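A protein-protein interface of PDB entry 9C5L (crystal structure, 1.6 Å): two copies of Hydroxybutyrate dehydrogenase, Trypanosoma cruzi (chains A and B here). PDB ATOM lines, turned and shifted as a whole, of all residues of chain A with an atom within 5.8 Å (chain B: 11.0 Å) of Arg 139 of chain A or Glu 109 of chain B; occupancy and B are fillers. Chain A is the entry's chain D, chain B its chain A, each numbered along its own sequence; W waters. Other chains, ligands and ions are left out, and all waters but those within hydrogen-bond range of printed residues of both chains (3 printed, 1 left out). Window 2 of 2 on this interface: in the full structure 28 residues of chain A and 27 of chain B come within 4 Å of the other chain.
N of Val 108 of chain B sits at hydrogen-bond distance from OE1 of Glu 181 of chain A (2.9 Å).
O of Phe 111 of chain B sits at hydrogen-bond distance from NE2 of Gln 132 of chain A, at 2.9 Å.
The guanidinium group of Arg 139 of chain A is in salt-bridge range of the side-chain carboxylate of Glu 109 of chain B, at 2.5 Å.
The side-chain amide nitrogen (NE2) of Gln 132 of chain A is in hydrogen-bond range of the backbone carbonyl oxygen (O) of Val 108 of chain B, at 2.8 Å.
N of Asn 160 of chain B lies within hydrogen-bond range of OE2 of Glu 181 of chain A.
The backbone carbonyl oxygen (O) of Glu 181 of chain A is in hydrogen-bond range of the guanidinium group (NH2) of Arg 139 of chain A (3.0 Å).
O of Asn 160 of chain B is in hydrogen-bond range of N of Ser 106 of chain B, at 2.9 Å.
Among the printed residues, merely in contact across the chains: Gln 132 of chain A with Glu 109 of chain B (3.3 Å), Leu 135 of chain A with Glu 109 of chain B (3.7 Å), Glu 181 of chain A with Pro 107 of chain B (3.6 Å) and Glu 181 of chain A with Met 159 of chain B (3.9 Å).
Arg 139 of chain A touches one residue of chain B.
Of chain B, only Val 108 (2.8 Å), Glu 109 (3.3 Å) and Phe 111 (2.9 Å) come within 4 Å of Gln 132 of chain A.
Leu 135 of chain A touches just one residue of chain B: Glu 109 (3.7 Å).
No residue of chain B comes within 4 Å of Pro 136 of chain A.
No residue of chain B comes within 4 Å of Gln 140 of chain A.
No residue of chain B comes within 4 Å of Gly 142 of chain A.
Glu 181 of chain A touches just these residues of chain B: Pro 107, Val 108, Met 159 and Asn 160.
No residue of chain B comes within 4 Å of Thr 182 of chain A.
Of the printed residues of chain A, Phe 111 of chain B touches Gln 132 (2.9 Å).
Of the printed residues of chain A, Asn 160 of chain B touches Glu 181 (2.7 Å).
Of the printed residues of chain A, Met 159 of chain B touches Glu 181 (3.9 Å).
Thr 185 of chain A touches none of the printed residues of chain B.
The nearest residue of chain B that does not touch Arg 139 of chain A is Pro 107 of chain B (6.3 Å).
The nearest residue of chain A that does not touch Glu 109 of chain B is Glu 181 of chain A (4.3 Å).
The nearest printed residue of chain A that does not touch Phe 111 of chain B is Glu 181 of chain A (6.4 Å).
Hydrophobic or aromatic side chains of chain B that line the printed part of chain A: Val 108, Phe 111 and Met 159.
Along chain B the printed residues that touch a printed residue of chain A span positions 107 to 160.
Among the printed residues, Asp or Glu carboxylates within 4 Å of a Lys or Arg side-chain nitrogen of the other chain: Arg 139 of chain A with Glu 109 of chain B (2.5 Å).
No position is printed for both chains.
Water W1 lies within hydrogen-bond range of OE1 of Glu 109 of chain B, OE1 of Glu 181 of chain A and NH2 of Arg 139 of chain A.
Water W3 lies within hydrogen-bond range of the side-chain hydroxyl of Ser 162 of chain B, the side-chain carboxylate of Glu 181 of chain A, the backbone carbonyl oxygen of Ser 106 of chain B and the backbone NH of Lys 161 of chain B.
Water W2 lies within hydrogen-bond range of O of Glu 181 of chain A (3.5 Å) and SD of Met 159 of chain B (3.6 Å).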
ATOM      1  N   GLN A 132     -21.847 -10.859  13.775  1.00  0.00           N
ATOM      2  CA  GLN A 132     -21.291 -10.529  12.470  1.00  0.00           C
ATOM      3  C   GLN A 132     -22.127  -9.488  11.751  1.00  0.00           C
ATOM      4  O   GLN A 132     -21.580  -8.588  11.097  1.00  0.00           O
ATOM      5  CB  GLN A 132     -21.191 -11.809  11.626  1.00  0.00           C
ATOM      6  CG  GLN A 132     -20.419 -11.668  10.358  1.00  0.00           C
ATOM      7  CD  GLN A 132     -20.154 -13.036   9.725  1.00  0.00           C
ATOM      8  OE1 GLN A 132     -21.085 -13.712   9.276  1.00  0.00           O
ATOM      9  NE2 GLN A 132     -18.897 -13.443   9.704  1.00  0.00           N
ATOM     10  N   CYS A 134     -24.183  -7.243  13.075  1.00  0.00           N
ATOM     11  CA  CYS A 134     -24.326  -5.965  13.788  1.00  0.00           C
ATOM     12  C   CYS A 134     -23.023  -5.187  13.913  1.00  0.00           C
ATOM     13  O   CYS A 134     -23.066  -3.965  14.119  1.00  0.00           O
ATOM     14  CB  CYS A 134     -24.880  -6.201  15.199  1.00  0.00           C
ATOM     15  SG  CYS A 134     -26.605  -6.702  15.206  1.00  0.00           S
ATOM     16  N   LEU A 135     -21.872  -5.853  13.850  1.00  0.00           N
ATOM     17  CA  LEU A 135     -20.618  -5.146  14.114  1.00  0.00           C
ATOM     18  C   LEU A 135     -20.319  -4.026  13.122  1.00  0.00           C
ATOM     19  O   LEU A 135     -19.797  -2.984  13.561  1.00  0.00           O
ATOM     20  CB  LEU A 135     -19.454  -6.141  14.159  1.00  0.00           C
ATOM     21  CG  LEU A 135     -19.220  -6.807  15.497  1.00  0.00           C
ATOM     22  CD1 LEU A 135     -18.286  -7.986  15.328  1.00  0.00           C
ATOM     23  CD2 LEU A 135     -18.646  -5.828  16.510  1.00  0.00           C
ATOM     24  N   PRO A 136     -20.595  -4.157  11.816  1.00  0.00           N
ATOM     25  CA  PRO A 136     -20.233  -3.059  10.883  1.00  0.00           C
ATOM     26  C   PRO A 136     -20.843  -1.718  11.260  1.00  0.00           C
ATOM     27  O   PRO A 136     -20.137  -0.697  11.291  1.00  0.00           O
ATOM     28  CB  PRO A 136     -20.746  -3.572   9.530  1.00  0.00           C
ATOM     29  CG  PRO A 136     -20.655  -5.073   9.682  1.00  0.00           C
ATOM     30  CD  PRO A 136     -21.029  -5.375  11.088  1.00  0.00           C
ATOM     31  N   SER A 137     -22.139  -1.700  11.588  1.00  0.00           N
ATOM     32  CA  SER A 137     -22.776  -0.451  11.991  1.00  0.00           C
ATOM     33  C   SER A 137     -22.198   0.064  13.302  1.00  0.00           C
ATOM     34  O   SER A 137     -22.004   1.276  13.467  1.00  0.00           O
ATOM     35  CB  SER A 137     -24.288  -0.645  12.105  1.00  0.00           C
ATOM     36  OG  SER A 137     -24.899   0.508  12.662  1.00  0.00           O
ATOM     37  N   MET A 138     -21.917  -0.842  14.249  1.00  0.00           N
ATOM     38  CA  MET A 138     -21.344  -0.423  15.520  1.00  0.00           C
ATOM     39  C   MET A 138     -19.979   0.229  15.317  1.00  0.00           C
ATOM     40  O   MET A 138     -19.661   1.249  15.942  1.00  0.00           O
ATOM     41  CB  MET A 138     -21.228  -1.623  16.458  1.00  0.00           C
ATOM     42  CG  MET A 138     -22.555  -2.067  17.006  1.00  0.00           C
ATOM     43  SD  MET A 138     -22.413  -3.568  17.967  1.00  0.00           S
ATOM     44  CE  MET A 138     -24.104  -3.817  18.511  1.00  0.00           C
ATOM     45  N   ARG A 139     -19.153  -0.358  14.467  1.00  0.00           N
ATOM     46  CA  ARG A 139     -17.852   0.232  14.178  1.00  0.00           C
ATOM     47  C   ARG A 139     -17.998   1.589  13.508  1.00  0.00           C
ATOM     48  O   ARG A 139     -17.264   2.528  13.835  1.00  0.00           O
ATOM     49  CB  ARG A 139     -17.036  -0.709  13.302  1.00  0.00           C
ATOM     50  CG  ARG A 139     -16.440  -1.900  14.068  1.00  0.00           C
ATOM     51  CD  ARG A 139     -15.552  -2.713  13.145  1.00  0.00           C
ATOM     52  NE  ARG A 139     -14.953  -3.863  13.796  1.00  0.00           N
ATOM     53  CZ  ARG A 139     -13.892  -3.825  14.590  1.00  0.00           C
ATOM     54  NH1 ARG A 139     -13.324  -2.684  14.933  1.00  0.00           N
ATOM     55  NH2 ARG A 139     -13.380  -4.964  15.040  1.00  0.00           N
ATOM     56  N   GLN A 140     -18.949   1.718  12.583  1.00  0.00           N
ATOM     57  CA  GLN A 140     -19.156   2.998  11.916  1.00  0.00           C
ATOM     58  C   GLN A 140     -19.580   4.068  12.913  1.00  0.00           C
ATOM     59  O   GLN A 140     -19.112   5.208  12.839  1.00  0.00           O
ATOM     60  CB  GLN A 140     -20.182   2.844  10.794  1.00  0.00           C
ATOM     61  CG  GLN A 140     -19.905   3.702   9.566  1.00  0.00           C
ATOM     62  CD  GLN A 140     -20.523   3.128   8.294  1.00  0.00           C
ATOM     63  OE1 GLN A 140     -19.987   3.306   7.200  1.00  0.00           O
ATOM     64  NE2 GLN A 140     -21.653   2.435   8.437  1.00  0.00           N
ATOM     65  N   ARG A 141     -20.450   3.717  13.864  1.00  0.00           N
ATOM     66  CA  ARG A 141     -20.912   4.680  14.859  1.00  0.00           C
ATOM     67  C   ARG A 141     -19.929   4.870  16.010  1.00  0.00           C
ATOM     68  O   ARG A 141     -20.033   5.873  16.735  1.00  0.00           O
ATOM     69  CB  ARG A 141     -22.264   4.241  15.425  1.00  0.00           C
ATOM     70  CG  ARG A 141     -23.419   4.367  14.449  1.00  0.00           C
ATOM     71  CD  ARG A 141     -24.212   5.653  14.702  1.00  0.00           C
ATOM     72  NE  ARG A 141     -25.518   5.625  14.053  1.00  0.00           N
ATOM     73  CZ  ARG A 141     -26.645   5.255  14.646  1.00  0.00           C
ATOM     74  NH1 ARG A 141     -26.670   4.888  15.917  1.00  0.00           N
ATOM     75  NH2 ARG A 141     -27.777   5.257  13.946  1.00  0.00           N
ATOM     76  N   GLY A 142     -18.980   3.958  16.185  1.00  0.00           N
ATOM     77  CA  GLY A 142     -18.043   4.036  17.285  1.00  0.00           C
ATOM     78  C   GLY A 142     -18.582   3.654  18.639  1.00  0.00           C
ATOM     79  O   GLY A 142     -18.000   4.036  19.657  1.00  0.00           O
ATOM     80  N   TRP A 143     -19.667   2.894  18.693  1.00  0.00           N
ATOM     81  CA  TRP A 143     -20.253   2.495  19.961  1.00  0.00           C
ATOM     82  C   TRP A 143     -21.012   1.194  19.754  1.00  0.00           C
ATOM     83  O   TRP A 143     -21.626   0.994  18.708  1.00  0.00           O
ATOM     84  CB  TRP A 143     -21.221   3.566  20.513  1.00  0.00           C
ATOM     85  CG  TRP A 143     -21.562   3.379  21.969  1.00  0.00           C
ATOM     86  CD1 TRP A 143     -20.898   3.912  23.044  1.00  0.00           C
ATOM     87  CD2 TRP A 143     -22.640   2.603  22.522  1.00  0.00           C
ATOM     88  NE1 TRP A 143     -21.487   3.512  24.212  1.00  0.00           N
ATOM     89  CE2 TRP A 143     -22.564   2.716  23.920  1.00  0.00           C
ATOM     90  CE3 TRP A 143     -23.664   1.836  21.967  1.00  0.00           C
ATOM     91  CZ2 TRP A 143     -23.462   2.085  24.773  1.00  0.00           C
ATOM     92  CZ3 TRP A 143     -24.569   1.226  22.833  1.00  0.00           C
ATOM     93  CH2 TRP A 143     -24.457   1.349  24.202  1.00  0.00           C
ATOM     94  N   GLU A 181     -10.982  -8.155  19.384  1.00  0.00           N
ATOM     95  CA  GLU A 181     -10.977  -7.524  18.075  1.00  0.00           C
ATOM     96  C   GLU A 181     -11.558  -6.114  18.097  1.00  0.00           C
ATOM     97  O   GLU A 181     -11.342  -5.366  17.142  1.00  0.00           O
ATOM     98  CB  GLU A 181     -11.763  -8.395  17.073  1.00  0.00           C
ATOM     99  CG  GLU A 181     -11.095  -9.735  16.783  1.00  0.00           C
ATOM    100  CD  GLU A 181     -11.784 -10.554  15.692  1.00  0.00           C
ATOM    101  OE1 GLU A 181     -12.679 -10.027  14.968  1.00  0.00           O
ATOM    102  OE2 GLU A 181     -11.416 -11.728  15.545  1.00  0.00           O
ATOM    103  N   THR A 182     -12.295  -5.748  19.154  1.00  0.00           N
ATOM    104  CA  THR A 182     -12.895  -4.427  19.279  1.00  0.00           C
ATOM    105  C   THR A 182     -12.306  -3.612  20.421  1.00  0.00           C
ATOM    106  O   THR A 182     -12.855  -2.559  20.759  1.00  0.00           O
ATOM    107  CB  THR A 182     -14.406  -4.533  19.477  1.00  0.00           C
ATOM    108  OG1 THR A 182     -14.714  -5.329  20.608  1.00  0.00           O
ATOM    109  CG2 THR A 182     -15.079  -5.090  18.206  1.00  0.00           C
ATOM    110  N   THR A 185     -11.961   0.230  20.428  1.00  0.00           N
ATOM    111  CA  THR A 185     -13.160   0.942  19.993  1.00  0.00           C
ATOM    112  C   THR A 185     -14.118   1.153  21.167  1.00  0.00           C
ATOM    113  O   THR A 185     -13.903   0.662  22.272  1.00  0.00           O
ATOM    114  CB  THR A 185     -13.882   0.156  18.887  1.00  0.00           C
ATOM    115  OG1 THR A 185     -14.628  -0.924  19.477  1.00  0.00           O
ATOM    116  CG2 THR A 185     -12.908  -0.379  17.864  1.00  0.00           C
ATOM    117  N   ILE A 187     -16.915  -0.264  21.251  1.00  0.00           N
ATOM    118  CA  ILE A 187     -17.694  -1.492  21.271  1.00  0.00           C
ATOM    119  C   ILE A 187     -17.107  -2.428  22.319  1.00  0.00           C
ATOM    120  O   ILE A 187     -15.909  -2.746  22.272  1.00  0.00           O
ATOM    121  CB  ILE A 187     -17.684  -2.178  19.892  1.00  0.00           C
ATOM    122  CG1 ILE A 187     -18.199  -1.259  18.793  1.00  0.00           C
ATOM    123  CG2 ILE A 187     -18.506  -3.476  19.942  1.00  0.00           C
ATOM    124  CD1 ILE A 187     -17.781  -1.755  17.402  1.00  0.00           C
ATOM    125  N   HIS B 104      -8.631 -21.387  10.723  1.00  0.00           N
ATOM    126  CA  HIS B 104      -8.850 -20.362   9.709  1.00  0.00           C
ATOM    127  C   HIS B 104      -8.800 -19.000  10.384  1.00  0.00           C
ATOM    128  O   HIS B 104      -9.601 -18.722  11.274  1.00  0.00           O
ATOM    129  CB  HIS B 104     -10.186 -20.544   8.990  1.00  0.00           C
ATOM    130  CG  HIS B 104     -10.404 -19.542   7.897  1.00  0.00           C
ATOM    131  ND1 HIS B 104      -9.829 -19.665   6.647  1.00  0.00           N
ATOM    132  CD2 HIS B 104     -11.095 -18.374   7.883  1.00  0.00           C
ATOM    133  CE1 HIS B 104     -10.167 -18.623   5.905  1.00  0.00           C
ATOM    134  NE2 HIS B 104     -10.926 -17.821   6.633  1.00  0.00           N
ATOM    135  N   VAL B 105      -7.891 -18.144   9.946  1.00  0.00           N
ATOM    136  CA  VAL B 105      -7.668 -16.837  10.554  1.00  0.00           C
ATOM    137  C   VAL B 105      -8.453 -15.795   9.761  1.00  0.00           C
ATOM    138  O   VAL B 105      -8.263 -15.645   8.545  1.00  0.00           O
ATOM    139  CB  VAL B 105      -6.163 -16.499  10.593  1.00  0.00           C
ATOM    140  CG1 VAL B 105      -5.939 -15.118  11.207  1.00  0.00           C
ATOM    141  CG2 VAL B 105      -5.404 -17.567  11.395  1.00  0.00           C
ATOM    142  N   SER B 106      -9.309 -15.037  10.465  1.00  0.00           N
ATOM    143  CA  SER B 106     -10.099 -13.997   9.842  1.00  0.00           C
ATOM    144  C   SER B 106     -10.746 -13.144  10.920  1.00  0.00           C
ATOM    145  O   SER B 106     -11.175 -13.699  11.926  1.00  0.00           O
ATOM    146  CB  SER B 106     -11.189 -14.598   8.967  1.00  0.00           C
ATOM    147  OG  SER B 106     -12.126 -13.596   8.595  1.00  0.00           O
ATOM    148  N   PRO B 107     -10.910 -11.833  10.708  1.00  0.00           N
ATOM    149  CA  PRO B 107     -11.743 -11.052  11.637  1.00  0.00           C
ATOM    150  C   PRO B 107     -13.166 -11.586  11.627  1.00  0.00           C
ATOM    151  O   PRO B 107     -13.614 -12.224  10.665  1.00  0.00           O
ATOM    152  CB  PRO B 107     -11.681  -9.617  11.091  1.00  0.00           C
ATOM    153  CG  PRO B 107     -10.588  -9.621  10.057  1.00  0.00           C
ATOM    154  CD  PRO B 107     -10.387 -11.022   9.597  1.00  0.00           C
ATOM    155  N   VAL B 108     -13.898 -11.282  12.703  1.00  0.00           N
ATOM    156  CA  VAL B 108     -15.233 -11.851  12.862  1.00  0.00           C
ATOM    157  C   VAL B 108     -16.173 -11.365  11.768  1.00  0.00           C
ATOM    158  O   VAL B 108     -17.009 -12.126  11.278  1.00  0.00           O
ATOM    159  CB  VAL B 108     -15.791 -11.513  14.260  1.00  0.00           C
ATOM    160  CG1 VAL B 108     -17.242 -11.948  14.378  1.00  0.00           C
ATOM    161  CG2 VAL B 108     -14.958 -12.153  15.343  1.00  0.00           C
ATOM    162  N   GLU B 109     -16.060 -10.093  11.366  1.00  0.00           N
ATOM    163  CA  GLU B 109     -17.047  -9.529  10.444  1.00  0.00           C
ATOM    164  C   GLU B 109     -17.053 -10.235   9.096  1.00  0.00           C
ATOM    165  O   GLU B 109     -18.086 -10.285   8.418  1.00  0.00           O
ATOM    166  CB  GLU B 109     -16.789  -8.036  10.205  1.00  0.00           C
ATOM    167  CG  GLU B 109     -17.061  -7.130  11.394  1.00  0.00           C
ATOM    168  CD  GLU B 109     -15.855  -7.003  12.311  1.00  0.00           C
ATOM    169  OE1 GLU B 109     -14.856  -7.731  12.091  1.00  0.00           O
ATOM    170  OE2 GLU B 109     -15.890  -6.164  13.247  1.00  0.00           O
ATOM    171  N   THR B 110     -15.901 -10.716   8.654  1.00  0.00           N
ATOM    172  CA  THR B 110     -15.768 -11.342   7.343  1.00  0.00           C
ATOM    173  C   THR B 110     -15.510 -12.838   7.444  1.00  0.00           C
ATOM    174  O   THR B 110     -15.217 -13.466   6.421  1.00  0.00           O
ATOM    175  CB  THR B 110     -14.630 -10.686   6.561  1.00  0.00           C
ATOM    176  OG1 THR B 110     -13.423 -10.785   7.335  1.00  0.00           O
ATOM    177  CG2 THR B 110     -14.944  -9.230   6.281  1.00  0.00           C
ATOM    178  N   PHE B 111     -15.636 -13.415   8.634  1.00  0.00           N
ATOM    179  CA  PHE B 111     -15.363 -14.838   8.825  1.00  0.00           C
ATOM    180  C   PHE B 111     -16.346 -15.643   7.978  1.00  0.00           C
ATOM    181  O   PHE B 111     -17.563 -15.497   8.162  1.00  0.00           O
ATOM    182  CB  PHE B 111     -15.478 -15.196  10.309  1.00  0.00           C
ATOM    183  CG  PHE B 111     -14.651 -16.381  10.696  1.00  0.00           C
ATOM    184  CD1 PHE B 111     -15.015 -17.646  10.303  1.00  0.00           C
ATOM    185  CD2 PHE B 111     -13.498 -16.230  11.447  1.00  0.00           C
ATOM    186  CE1 PHE B 111     -14.245 -18.743  10.652  1.00  0.00           C
ATOM    187  CE2 PHE B 111     -12.729 -17.301  11.791  1.00  0.00           C
ATOM    188  CZ  PHE B 111     -13.099 -18.587  11.389  1.00  0.00           C
ATOM    189  N   PRO B 112     -15.878 -16.490   7.051  1.00  0.00           N
ATOM    190  CA  PRO B 112     -16.821 -17.208   6.177  1.00  0.00           C
ATOM    191  C   PRO B 112     -17.662 -18.186   6.972  1.00  0.00           C
ATOM    192  O   PRO B 112     -17.163 -18.885   7.849  1.00  0.00           O
ATOM    193  CB  PRO B 112     -15.911 -17.938   5.178  1.00  0.00           C
ATOM    194  CG  PRO B 112     -14.625 -17.180   5.198  1.00  0.00           C
ATOM    195  CD  PRO B 112     -14.478 -16.709   6.636  1.00  0.00           C
ATOM    196  N   SER B 113     -18.949 -18.252   6.625  1.00  0.00           N
ATOM    197  CA  SER B 113     -19.874 -19.111   7.361  1.00  0.00           C
ATOM    198  C   SER B 113     -19.484 -20.583   7.250  1.00  0.00           C
ATOM    199  O   SER B 113     -19.522 -21.325   8.246  1.00  0.00           O
ATOM    200  CB  SER B 113     -21.298 -18.905   6.834  1.00  0.00           C
ATOM    201  OG  SER B 113     -22.162 -19.926   7.301  1.00  0.00           O
ATOM    202  N   TRP B 116     -16.531 -21.283   9.564  1.00  0.00           N
ATOM    203  CA  TRP B 116     -17.010 -21.386  10.932  1.00  0.00           C
ATOM    204  C   TRP B 116     -17.598 -22.770  11.186  1.00  0.00           C
ATOM    205  O   TRP B 116     -17.201 -23.460  12.142  1.00  0.00           O
ATOM    206  CB  TRP B 116     -18.057 -20.289  11.220  1.00  0.00           C
ATOM    207  CG  TRP B 116     -18.687 -20.433  12.584  1.00  0.00           C
ATOM    208  CD1 TRP B 116     -19.717 -21.279  12.932  1.00  0.00           C
ATOM    209  CD2 TRP B 116     -18.355 -19.702  13.773  1.00  0.00           C
ATOM    210  NE1 TRP B 116     -20.009 -21.129  14.265  1.00  0.00           N
ATOM    211  CE2 TRP B 116     -19.194 -20.166  14.802  1.00  0.00           C
ATOM    212  CE3 TRP B 116     -17.418 -18.705  14.070  1.00  0.00           C
ATOM    213  CZ2 TRP B 116     -19.119 -19.678  16.111  1.00  0.00           C
ATOM    214  CZ3 TRP B 116     -17.343 -18.213  15.368  1.00  0.00           C
ATOM    215  CH2 TRP B 116     -18.189 -18.700  16.381  1.00  0.00           C
ATOM    216  N   MET B 159      -7.252 -12.611  18.831  1.00  0.00           N
ATOM    217  CA  MET B 159      -7.854 -11.942  17.691  1.00  0.00           C
ATOM    218  C   MET B 159      -7.818 -12.836  16.459  1.00  0.00           C
ATOM    219  O   MET B 159      -6.839 -13.547  16.211  1.00  0.00           O
ATOM    220  CB  MET B 159      -7.121 -10.631  17.392  1.00  0.00           C
ATOM    221  CG  MET B 159      -7.399  -9.575  18.417  1.00  0.00           C
ATOM    222  SD  MET B 159      -6.656  -7.989  17.963  1.00  0.00           S
ATOM    223  CE  MET B 159      -4.940  -8.333  18.211  1.00  0.00           C
ATOM    224  N   ASN B 160      -8.887 -12.746  15.662  1.00  0.00           N
ATOM    225  CA  ASN B 160      -9.013 -13.343  14.338  1.00  0.00           C
ATOM    226  C   ASN B 160      -9.163 -14.849  14.382  1.00  0.00           C
ATOM    227  O   ASN B 160      -9.043 -15.495  13.348  1.00  0.00           O
ATOM    228  CB  ASN B 160      -7.834 -12.953  13.444  1.00  0.00           C
ATOM    229  CG  ASN B 160      -7.720 -11.455  13.290  1.00  0.00           C
ATOM    230  OD1 ASN B 160      -8.726 -10.771  13.151  1.00  0.00           O
ATOM    231  ND2 ASN B 160      -6.498 -10.940  13.335  1.00  0.00           N
ATOM    232  N   LYS B 161      -9.487 -15.412  15.548  1.00  0.00           N
ATOM    233  CA  LYS B 161      -9.635 -16.837  15.707  1.00  0.00           C
ATOM    234  C   LYS B 161     -10.940 -17.157  16.427  1.00  0.00           C
ATOM    235  O   LYS B 161     -11.001 -18.082  17.239  1.00  0.00           O
ATOM    236  CB  LYS B 161      -8.424 -17.403  16.460  1.00  0.00           C
ATOM    237  CG  LYS B 161      -7.152 -17.391  15.586  1.00  0.00           C
ATOM    238  CD  LYS B 161      -5.902 -17.919  16.315  1.00  0.00           C
ATOM    239  CE  LYS B 161      -4.741 -17.973  15.331  1.00  0.00           C
ATOM    240  NZ  LYS B 161      -3.470 -18.419  15.965  1.00  0.00           N
ATOM    241  N   SER B 162     -12.022 -16.468  16.033  1.00  0.00           N
ATOM    242  CA  SER B 162     -13.293 -16.623  16.737  1.00  0.00           C
ATOM    243  C   SER B 162     -13.796 -18.067  16.674  1.00  0.00           C
ATOM    244  O   SER B 162     -14.153 -18.642  17.708  1.00  0.00           O
ATOM    245  CB  SER B 162     -14.332 -15.652  16.169  1.00  0.00           C
ATOM    246  OG  SER B 162     -14.475 -15.779  14.777  1.00  0.00           O
ATOM    247  N   ALA B 163     -13.850 -18.660  15.478  1.00  0.00           N
ATOM    248  CA  ALA B 163     -14.407 -20.010  15.371  1.00  0.00           C
ATOM    249  C   ALA B 163     -13.568 -21.007  16.160  1.00  0.00           C
ATOM    250  O   ALA B 163     -14.109 -21.868  16.862  1.00  0.00           O
ATOM    251  CB  ALA B 163     -14.493 -20.440  13.906  1.00  0.00           C
HETATM  252  O   HOH W   1     -12.954  -7.475  13.938  1.00  0.00           O
HETATM  253  O   HOH W   2      -8.243  -4.794  18.586  1.00  0.00           O
HETATM  254  O   HOH W   3     -12.435 -14.008  14.398  1.00  0.00           O
